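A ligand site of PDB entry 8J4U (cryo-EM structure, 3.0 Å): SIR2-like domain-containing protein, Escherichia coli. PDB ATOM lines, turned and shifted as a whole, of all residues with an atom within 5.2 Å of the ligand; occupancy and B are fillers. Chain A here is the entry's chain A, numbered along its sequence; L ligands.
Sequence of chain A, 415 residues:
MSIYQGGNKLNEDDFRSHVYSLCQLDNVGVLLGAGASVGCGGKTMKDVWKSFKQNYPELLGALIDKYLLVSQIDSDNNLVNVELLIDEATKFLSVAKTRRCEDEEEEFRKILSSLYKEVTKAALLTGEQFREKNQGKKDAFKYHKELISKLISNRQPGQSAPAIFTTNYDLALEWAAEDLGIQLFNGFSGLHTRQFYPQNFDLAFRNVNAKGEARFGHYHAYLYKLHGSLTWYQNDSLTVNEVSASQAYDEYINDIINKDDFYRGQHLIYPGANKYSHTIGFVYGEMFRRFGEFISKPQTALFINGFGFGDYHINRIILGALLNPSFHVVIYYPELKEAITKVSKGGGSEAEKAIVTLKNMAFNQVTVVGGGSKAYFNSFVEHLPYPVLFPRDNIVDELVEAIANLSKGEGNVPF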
ATOM      1  N   GLY A  33      20.425  18.260  28.872  1.00  0.00           N
ATOM      2  CA  GLY A  33      20.087  16.949  28.384  1.00  0.00           C
ATOM      3  C   GLY A  33      18.848  16.370  29.040  1.00  0.00           C
ATOM      4  O   GLY A  33      18.066  17.099  29.650  1.00  0.00           O
ATOM      5  N   ALA A  34      18.684  15.051  28.932  1.00  0.00           N
ATOM      6  CA  ALA A  34      17.491  14.390  29.467  1.00  0.00           C
ATOM      7  C   ALA A  34      17.599  14.078  30.954  1.00  0.00           C
ATOM      8  O   ALA A  34      16.568  13.852  31.589  1.00  0.00           O
ATOM      9  CB  ALA A  34      17.213  13.102  28.708  1.00  0.00           C
ATOM     10  N   GLY A  35      18.806  14.048  31.505  1.00  0.00           N
ATOM     11  CA  GLY A  35      18.973  13.834  32.917  1.00  0.00           C
ATOM     12  C   GLY A  35      18.662  15.030  33.782  1.00  0.00           C
ATOM     13  O   GLY A  35      18.676  14.926  35.008  1.00  0.00           O
ATOM     14  N   ALA A  36      18.379  16.177  33.167  1.00  0.00           N
ATOM     15  CA  ALA A  36      18.022  17.386  33.893  1.00  0.00           C
ATOM     16  C   ALA A  36      16.554  17.438  34.280  1.00  0.00           C
ATOM     17  O   ALA A  36      16.181  18.294  35.095  1.00  0.00           O
ATOM     18  CB  ALA A  36      18.374  18.615  33.061  1.00  0.00           C
ATOM     19  N   VAL A  38      14.682  14.673  35.453  1.00  0.00           N
ATOM     20  CA  VAL A  38      14.265  13.556  36.293  1.00  0.00           C
ATOM     21  C   VAL A  38      13.877  14.016  37.685  1.00  0.00           C
ATOM     22  O   VAL A  38      13.240  13.241  38.428  1.00  0.00           O
ATOM     23  CB  VAL A  38      15.359  12.488  36.419  1.00  0.00           C
ATOM     24  CG1 VAL A  38      15.848  12.075  35.058  1.00  0.00           C
ATOM     25  CG2 VAL A  38      16.501  12.989  37.248  1.00  0.00           C
ATOM     26  N   THR A  44      15.108   8.813  32.224  1.00  0.00           N
ATOM     27  CA  THR A  44      16.258   8.695  31.340  1.00  0.00           C
ATOM     28  C   THR A  44      15.938   7.749  30.186  1.00  0.00           C
ATOM     29  O   THR A  44      14.814   7.255  30.039  1.00  0.00           O
ATOM     30  CB  THR A  44      17.483   8.218  32.107  1.00  0.00           C
ATOM     31  OG1 THR A  44      17.211   6.948  32.719  1.00  0.00           O
ATOM     32  CG2 THR A  44      17.851   9.217  33.173  1.00  0.00           C
ATOM     33  N   MET A  45      16.940   7.494  29.350  1.00  0.00           N
ATOM     34  CA  MET A  45      16.753   6.724  28.130  1.00  0.00           C
ATOM     35  C   MET A  45      16.980   5.227  28.321  1.00  0.00           C
ATOM     36  O   MET A  45      16.592   4.449  27.454  1.00  0.00           O
ATOM     37  CB  MET A  45      17.685   7.254  27.038  1.00  0.00           C
ATOM     38  CG  MET A  45      17.367   6.746  25.647  1.00  0.00           C
ATOM     39  SD  MET A  45      15.667   7.034  25.127  1.00  0.00           S
ATOM     40  CE  MET A  45      15.530   8.814  25.253  1.00  0.00           C
ATOM     41  N   ASN A  81      20.190   3.331  21.045  1.00  0.00           N
ATOM     42  CA  ASN A  81      19.752   4.682  20.708  1.00  0.00           C
ATOM     43  C   ASN A  81      18.323   4.610  20.173  1.00  0.00           C
ATOM     44  O   ASN A  81      18.058   3.866  19.228  1.00  0.00           O
ATOM     45  CB  ASN A  81      20.688   5.310  19.687  1.00  0.00           C
ATOM     46  CG  ASN A  81      20.740   6.819  19.802  1.00  0.00           C
ATOM     47  OD1 ASN A  81      19.746   7.463  20.081  1.00  0.00           O
ATOM     48  ND2 ASN A  81      21.917   7.389  19.562  1.00  0.00           N
ATOM     49  N   GLU A  83      16.334   7.210  19.004  1.00  0.00           N
ATOM     50  CA  GLU A  83      15.940   8.106  17.924  1.00  0.00           C
ATOM     51  C   GLU A  83      16.223   7.506  16.554  1.00  0.00           C
ATOM     52  O   GLU A  83      15.392   7.573  15.642  1.00  0.00           O
ATOM     53  CB  GLU A  83      16.681   9.437  18.065  1.00  0.00           C
ATOM     54  CG  GLU A  83      16.256  10.268  19.258  1.00  0.00           C
ATOM     55  CD  GLU A  83      16.952   9.867  20.537  1.00  0.00           C
ATOM     56  OE1 GLU A  83      17.733   8.901  20.519  1.00  0.00           O
ATOM     57  OE2 GLU A  83      16.711  10.520  21.574  1.00  0.00           O
ATOM     58  N   THR A 167      18.147  18.942  24.376  1.00  0.00           N
ATOM     59  CA  THR A 167      17.771  17.782  23.604  1.00  0.00           C
ATOM     60  C   THR A 167      16.416  17.209  24.006  1.00  0.00           C
ATOM     61  O   THR A 167      15.935  16.288  23.341  1.00  0.00           O
ATOM     62  CB  THR A 167      18.828  16.674  23.743  1.00  0.00           C
ATOM     63  OG1 THR A 167      19.166  16.500  25.119  1.00  0.00           O
ATOM     64  CG2 THR A 167      20.064  17.022  22.957  1.00  0.00           C
ATOM     65  N   HIS A 227      15.702  18.609  18.845  1.00  0.00           N
ATOM     66  CA  HIS A 227      14.998  17.382  18.478  1.00  0.00           C
ATOM     67  C   HIS A 227      13.494  17.563  18.363  1.00  0.00           C
ATOM     68  O   HIS A 227      12.786  16.573  18.141  1.00  0.00           O
ATOM     69  CB  HIS A 227      15.308  16.267  19.485  1.00  0.00           C
ATOM     70  CG  HIS A 227      16.633  15.614  19.265  1.00  0.00           C
ATOM     71  ND1 HIS A 227      17.354  15.048  20.296  1.00  0.00           N
ATOM     72  CD2 HIS A 227      17.371  15.418  18.147  1.00  0.00           C
ATOM     73  CE1 HIS A 227      18.475  14.547  19.818  1.00  0.00           C
ATOM     74  NE2 HIS A 227      18.513  14.756  18.517  1.00  0.00           N
ATOM     75  N   ASN A 305      25.604  19.893  31.021  1.00  0.00           N
ATOM     76  CA  ASN A 305      25.007  19.198  32.143  1.00  0.00           C
ATOM     77  C   ASN A 305      23.878  18.301  31.637  1.00  0.00           C
ATOM     78  O   ASN A 305      23.070  18.740  30.810  1.00  0.00           O
ATOM     79  CB  ASN A 305      24.472  20.182  33.182  1.00  0.00           C
ATOM     80  CG  ASN A 305      23.609  19.519  34.233  1.00  0.00           C
ATOM     81  OD1 ASN A 305      22.598  18.882  33.936  1.00  0.00           O
ATOM     82  ND2 ASN A 305      24.002  19.667  35.484  1.00  0.00           N
ATOM     83  N   GLY A 306      23.831  17.068  32.131  1.00  0.00           N
ATOM     84  CA  GLY A 306      22.768  16.158  31.800  1.00  0.00           C
ATOM     85  C   GLY A 306      23.006  15.316  30.567  1.00  0.00           C
ATOM     86  O   GLY A 306      22.151  14.485  30.237  1.00  0.00           O
ATOM     87  N   PHE A 307      24.123  15.497  29.884  1.00  0.00           N
ATOM     88  CA  PHE A 307      24.340  14.983  28.534  1.00  0.00           C
ATOM     89  C   PHE A 307      25.354  13.861  28.581  1.00  0.00           C
ATOM     90  O   PHE A 307      26.472  14.042  29.080  1.00  0.00           O
ATOM     91  CB  PHE A 307      24.804  16.114  27.621  1.00  0.00           C
ATOM     92  CG  PHE A 307      25.095  15.682  26.217  1.00  0.00           C
ATOM     93  CD1 PHE A 307      24.101  15.164  25.414  1.00  0.00           C
ATOM     94  CD2 PHE A 307      26.371  15.819  25.700  1.00  0.00           C
ATOM     95  CE1 PHE A 307      24.376  14.787  24.122  1.00  0.00           C
ATOM     96  CE2 PHE A 307      26.651  15.435  24.409  1.00  0.00           C
ATOM     97  CZ  PHE A 307      25.656  14.915  23.620  1.00  0.00           C
ATOM     98  N   GLY A 308      24.965  12.688  28.071  1.00  0.00           N
ATOM     99  CA  GLY A 308      25.874  11.578  27.881  1.00  0.00           C
ATOM    100  C   GLY A 308      26.445  11.626  26.472  1.00  0.00           C
ATOM    101  O   GLY A 308      25.695  11.708  25.490  1.00  0.00           O
ATOM    102  N   GLY A 310      27.160  10.340  23.836  1.00  0.00           N
ATOM    103  CA  GLY A 310      26.906   9.254  22.920  1.00  0.00           C
ATOM    104  C   GLY A 310      26.479   9.722  21.545  1.00  0.00           C
ATOM    105  O   GLY A 310      25.763   9.004  20.834  1.00  0.00           O
ATOM    106  N   ASP A 311      26.893  10.920  21.159  1.00  0.00           N
ATOM    107  CA  ASP A 311      26.622  11.487  19.847  1.00  0.00           C
ATOM    108  C   ASP A 311      27.934  11.834  19.175  1.00  0.00           C
ATOM    109  O   ASP A 311      28.806  12.461  19.788  1.00  0.00           O
ATOM    110  CB  ASP A 311      25.738  12.731  19.956  1.00  0.00           C
ATOM    111  CG  ASP A 311      25.279  13.248  18.607  1.00  0.00           C
ATOM    112  OD1 ASP A 311      26.135  13.497  17.737  1.00  0.00           O
ATOM    113  OD2 ASP A 311      24.050  13.401  18.406  1.00  0.00           O
ATOM    114  N   ILE A 314      28.130  16.055  17.752  1.00  0.00           N
ATOM    115  CA  ILE A 314      28.341  17.105  18.745  1.00  0.00           C
ATOM    116  C   ILE A 314      29.758  17.031  19.296  1.00  0.00           C
ATOM    117  O   ILE A 314      30.378  18.065  19.580  1.00  0.00           O
ATOM    118  CB  ILE A 314      27.282  17.003  19.859  1.00  0.00           C
ATOM    119  CG1 ILE A 314      25.901  17.279  19.281  1.00  0.00           C
ATOM    120  CG2 ILE A 314      27.581  17.985  20.974  1.00  0.00           C
ATOM    121  CD1 ILE A 314      24.772  16.999  20.222  1.00  0.00           C
ATOM    122  N   TYR A 333      29.930  15.174  34.930  1.00  0.00           N
ATOM    123  CA  TYR A 333      29.798  13.754  34.618  1.00  0.00           C
ATOM    124  C   TYR A 333      29.881  12.940  35.909  1.00  0.00           C
ATOM    125  O   TYR A 333      30.987  12.762  36.446  1.00  0.00           O
ATOM    126  CB  TYR A 333      30.868  13.323  33.623  1.00  0.00           C
ATOM    127  CG  TYR A 333      30.617  12.001  32.948  1.00  0.00           C
ATOM    128  CD1 TYR A 333      29.941  11.927  31.745  1.00  0.00           C
ATOM    129  CD2 TYR A 333      31.073  10.822  33.517  1.00  0.00           C
ATOM    130  CE1 TYR A 333      29.714  10.718  31.123  1.00  0.00           C
ATOM    131  CE2 TYR A 333      30.856   9.607  32.902  1.00  0.00           C
ATOM    132  CZ  TYR A 333      30.174   9.553  31.708  1.00  0.00           C
ATOM    133  OH  TYR A 333      29.951   8.347  31.094  1.00  0.00           O
ATOM    134  N   PRO A 334      28.765  12.423  36.427  1.00  0.00           N
ATOM    135  CA  PRO A 334      28.784  11.831  37.769  1.00  0.00           C
ATOM    136  C   PRO A 334      29.173  10.348  37.841  1.00  0.00           C
ATOM    137  O   PRO A 334      28.970   9.724  38.887  1.00  0.00           O
ATOM    138  CB  PRO A 334      27.345  12.023  38.256  1.00  0.00           C
ATOM    139  CG  PRO A 334      26.531  12.085  37.037  1.00  0.00           C
ATOM    140  CD  PRO A 334      27.395  12.603  35.930  1.00  0.00           C
ATOM    141  N   GLU A 335      29.730   9.793  36.768  1.00  0.00           N
ATOM    142  CA  GLU A 335      30.195   8.409  36.752  1.00  0.00           C
ATOM    143  C   GLU A 335      31.586   8.338  36.148  1.00  0.00           C
ATOM    144  O   GLU A 335      31.866   7.518  35.265  1.00  0.00           O
ATOM    145  CB  GLU A 335      29.217   7.513  36.002  1.00  0.00           C
ATOM    146  CG  GLU A 335      28.008   7.108  36.819  1.00  0.00           C
ATOM    147  CD  GLU A 335      26.815   6.707  35.970  1.00  0.00           C
ATOM    148  OE1 GLU A 335      26.771   7.097  34.785  1.00  0.00           O
ATOM    149  OE2 GLU A 335      25.931   6.001  36.491  1.00  0.00           O
ATOM    150  N   ALA A 375      27.449  16.258  41.115  1.00  0.00           N
ATOM    151  CA  ALA A 375      27.470  16.732  39.732  1.00  0.00           C
ATOM    152  C   ALA A 375      26.069  16.796  39.139  1.00  0.00           C
ATOM    153  O   ALA A 375      25.922  16.813  37.918  1.00  0.00           O
ATOM    154  CB  ALA A 375      28.373  15.833  38.889  1.00  0.00           C
ATOM    155  N   TYR A 376      25.045  16.823  39.979  1.00  0.00           N
ATOM    156  CA  TYR A 376      23.673  16.837  39.525  1.00  0.00           C
ATOM    157  C   TYR A 376      23.196  18.267  39.281  1.00  0.00           C
ATOM    158  O   TYR A 376      23.865  19.247  39.606  1.00  0.00           O
ATOM    159  CB  TYR A 376      22.783  16.132  40.548  1.00  0.00           C
ATOM    160  CG  TYR A 376      22.810  14.617  40.461  1.00  0.00           C
ATOM    161  CD1 TYR A 376      23.747  13.963  39.674  1.00  0.00           C
ATOM    162  CD2 TYR A 376      21.899  13.841  41.164  1.00  0.00           C
ATOM    163  CE1 TYR A 376      23.778  12.586  39.591  1.00  0.00           C
ATOM    164  CE2 TYR A 376      21.917  12.468  41.087  1.00  0.00           C
ATOM    165  CZ  TYR A 376      22.854  11.838  40.304  1.00  0.00           C
ATOM    166  OH  TYR A 376      22.873  10.465  40.227  1.00  0.00           O
ATOM    167  N   PHE A 377      22.012  18.367  38.662  1.00  0.00           N
ATOM    168  CA  PHE A 377      21.485  19.659  38.231  1.00  0.00           C
ATOM    169  C   PHE A 377      21.314  20.615  39.413  1.00  0.00           C
ATOM    170  O   PHE A 377      21.740  21.777  39.346  1.00  0.00           O
ATOM    171  CB  PHE A 377      20.156  19.423  37.512  1.00  0.00           C
ATOM    172  CG  PHE A 377      19.559  20.651  36.901  1.00  0.00           C
ATOM    173  CD1 PHE A 377      20.174  21.280  35.843  1.00  0.00           C
ATOM    174  CD2 PHE A 377      18.356  21.153  37.378  1.00  0.00           C
ATOM    175  CE1 PHE A 377      19.614  22.395  35.278  1.00  0.00           C
ATOM    176  CE2 PHE A 377      17.796  22.268  36.813  1.00  0.00           C
ATOM    177  CZ  PHE A 377      18.422  22.893  35.763  1.00  0.00           C
HETATM  178  N1  LIG L   1      21.012  15.241  37.355  1.00  0.00           N
HETATM  179  C1  LIG L   1      21.984  15.367  36.437  1.00  0.00           C
HETATM  180  N2  LIG L   1      22.395  14.350  35.662  1.00  0.00           N
HETATM  181  C2  LIG L   1      21.828  13.133  35.752  1.00  0.00           C
HETATM  182  C3  LIG L   1      20.759  12.921  36.729  1.00  0.00           C
HETATM  183  C4  LIG L   1      20.365  14.082  37.560  1.00  0.00           C
HETATM  184  N3  LIG L   1      19.386  13.976  38.487  1.00  0.00           N
HETATM  185  N4  LIG L   1      20.387  11.635  36.614  1.00  0.00           N
HETATM  186  C5  LIG L   1      21.143  11.071  35.643  1.00  0.00           C
HETATM  187  N5  LIG L   1      22.023  11.961  35.138  1.00  0.00           N
HETATM  188  P1  LIG L   1      21.194   9.788  28.543  1.00  0.00           P
HETATM  189  P2  LIG L   1      21.049  11.886  26.668  1.00  0.00           P
HETATM  190  C6  LIG L   1      23.012  11.773  34.059  1.00  0.00           C
HETATM  191  O1  LIG L   1      21.349   8.317  28.258  1.00  0.00           O
HETATM  192  O2  LIG L   1      22.079  12.747  25.994  1.00  0.00           O
HETATM  193  C7  LIG L   1      20.637  10.330  21.273  1.00  0.00           C
HETATM  194  O3  LIG L   1      21.753   9.439  21.202  1.00  0.00           O
HETATM  195  C8  LIG L   1      23.624  10.377  33.969  1.00  0.00           C
HETATM  196  O4  LIG L   1      24.877  10.297  34.661  1.00  0.00           O
HETATM  197  O5  LIG L   1      19.844  10.338  28.920  1.00  0.00           O
HETATM  198  O6  LIG L   1      20.115  12.503  27.680  1.00  0.00           O
HETATM  199  C9  LIG L   1      21.080  11.745  20.932  1.00  0.00           C
HETATM  200  O7  LIG L   1      22.473  11.758  20.603  1.00  0.00           O
HETATM  201  C10 LIG L   1      23.805  10.130  32.486  1.00  0.00           C
HETATM  202  O8  LIG L   1      25.160  10.330  32.107  1.00  0.00           O
HETATM  203  O9  LIG L   1      21.780  10.595  27.284  1.00  0.00           O
HETATM  204  C11 LIG L   1      20.841  12.560  22.176  1.00  0.00           C
HETATM  205  O10 LIG L   1      21.950  13.419  22.461  1.00  0.00           O
HETATM  206  C12 LIG L   1      22.916  11.148  31.792  1.00  0.00           C
HETATM  207  O11 LIG L   1      22.351  11.975  32.800  1.00  0.00           O
HETATM  208  C13 LIG L   1      20.662  11.516  23.262  1.00  0.00           C
HETATM  209  O12 LIG L   1      20.141  10.366  22.614  1.00  0.00           O
HETATM  210  C14 LIG L   1      21.795  10.511  30.990  1.00  0.00           C
HETATM  211  O13 LIG L   1      22.256  10.199  29.682  1.00  0.00           O
HETATM  212  C15 LIG L   1      19.770  11.969  24.399  1.00  0.00           C
HETATM  213  O14 LIG L   1      20.140  11.214  25.538  1.00  0.00           O
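ND2 of Asn 81 is in hydrogen-bond range of O3 of the ligand (2.6 Å).
The backbone NH (N) of Ala 34 sits close to an oxygen (O6) of the ligand (3.2 Å).
An oxygen (O7) of the ligand sits at hydrogen-bond distance from the side-chain carboxylate of Asp 311.
OE1 of Glu 83 lies close to OD1 of Asn 81 (2.5 Å).
The side-chain carboxylate (OD1) of Asp 311 lies within hydrogen-bond range of the backbone NH (N) of Ile 314, 3.2 Å away.
The backbone carbonyl oxygen (O) of Gly 35 lies close to a nitrogen (N1) of the ligand (3.3 Å).
Merely in contact with the ligand: Phe 307 (3.2 Å), Val 38 (3.3 Å), Glu 83 (3.3 Å), Pro 334 (3.4 Å), Phe 377 (3.5 Å), Gly 308 (3.6 Å), Gly 306 (3.6 Å), Tyr 376 (3.6 Å), Glu 335 (3.7 Å) and His 227 (3.9 Å).
Hydrophobic or aromatic side chains within 4 Å of the ligand: Ala 34, Val 38, His 227, Phe 307, Pro 334 and Tyr 376.
Of the 24 residues printed, 14 come within 4 Å of the ligand.
The nearest printed residue that does not touch the ligand is Met 45 (4.01 Å).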
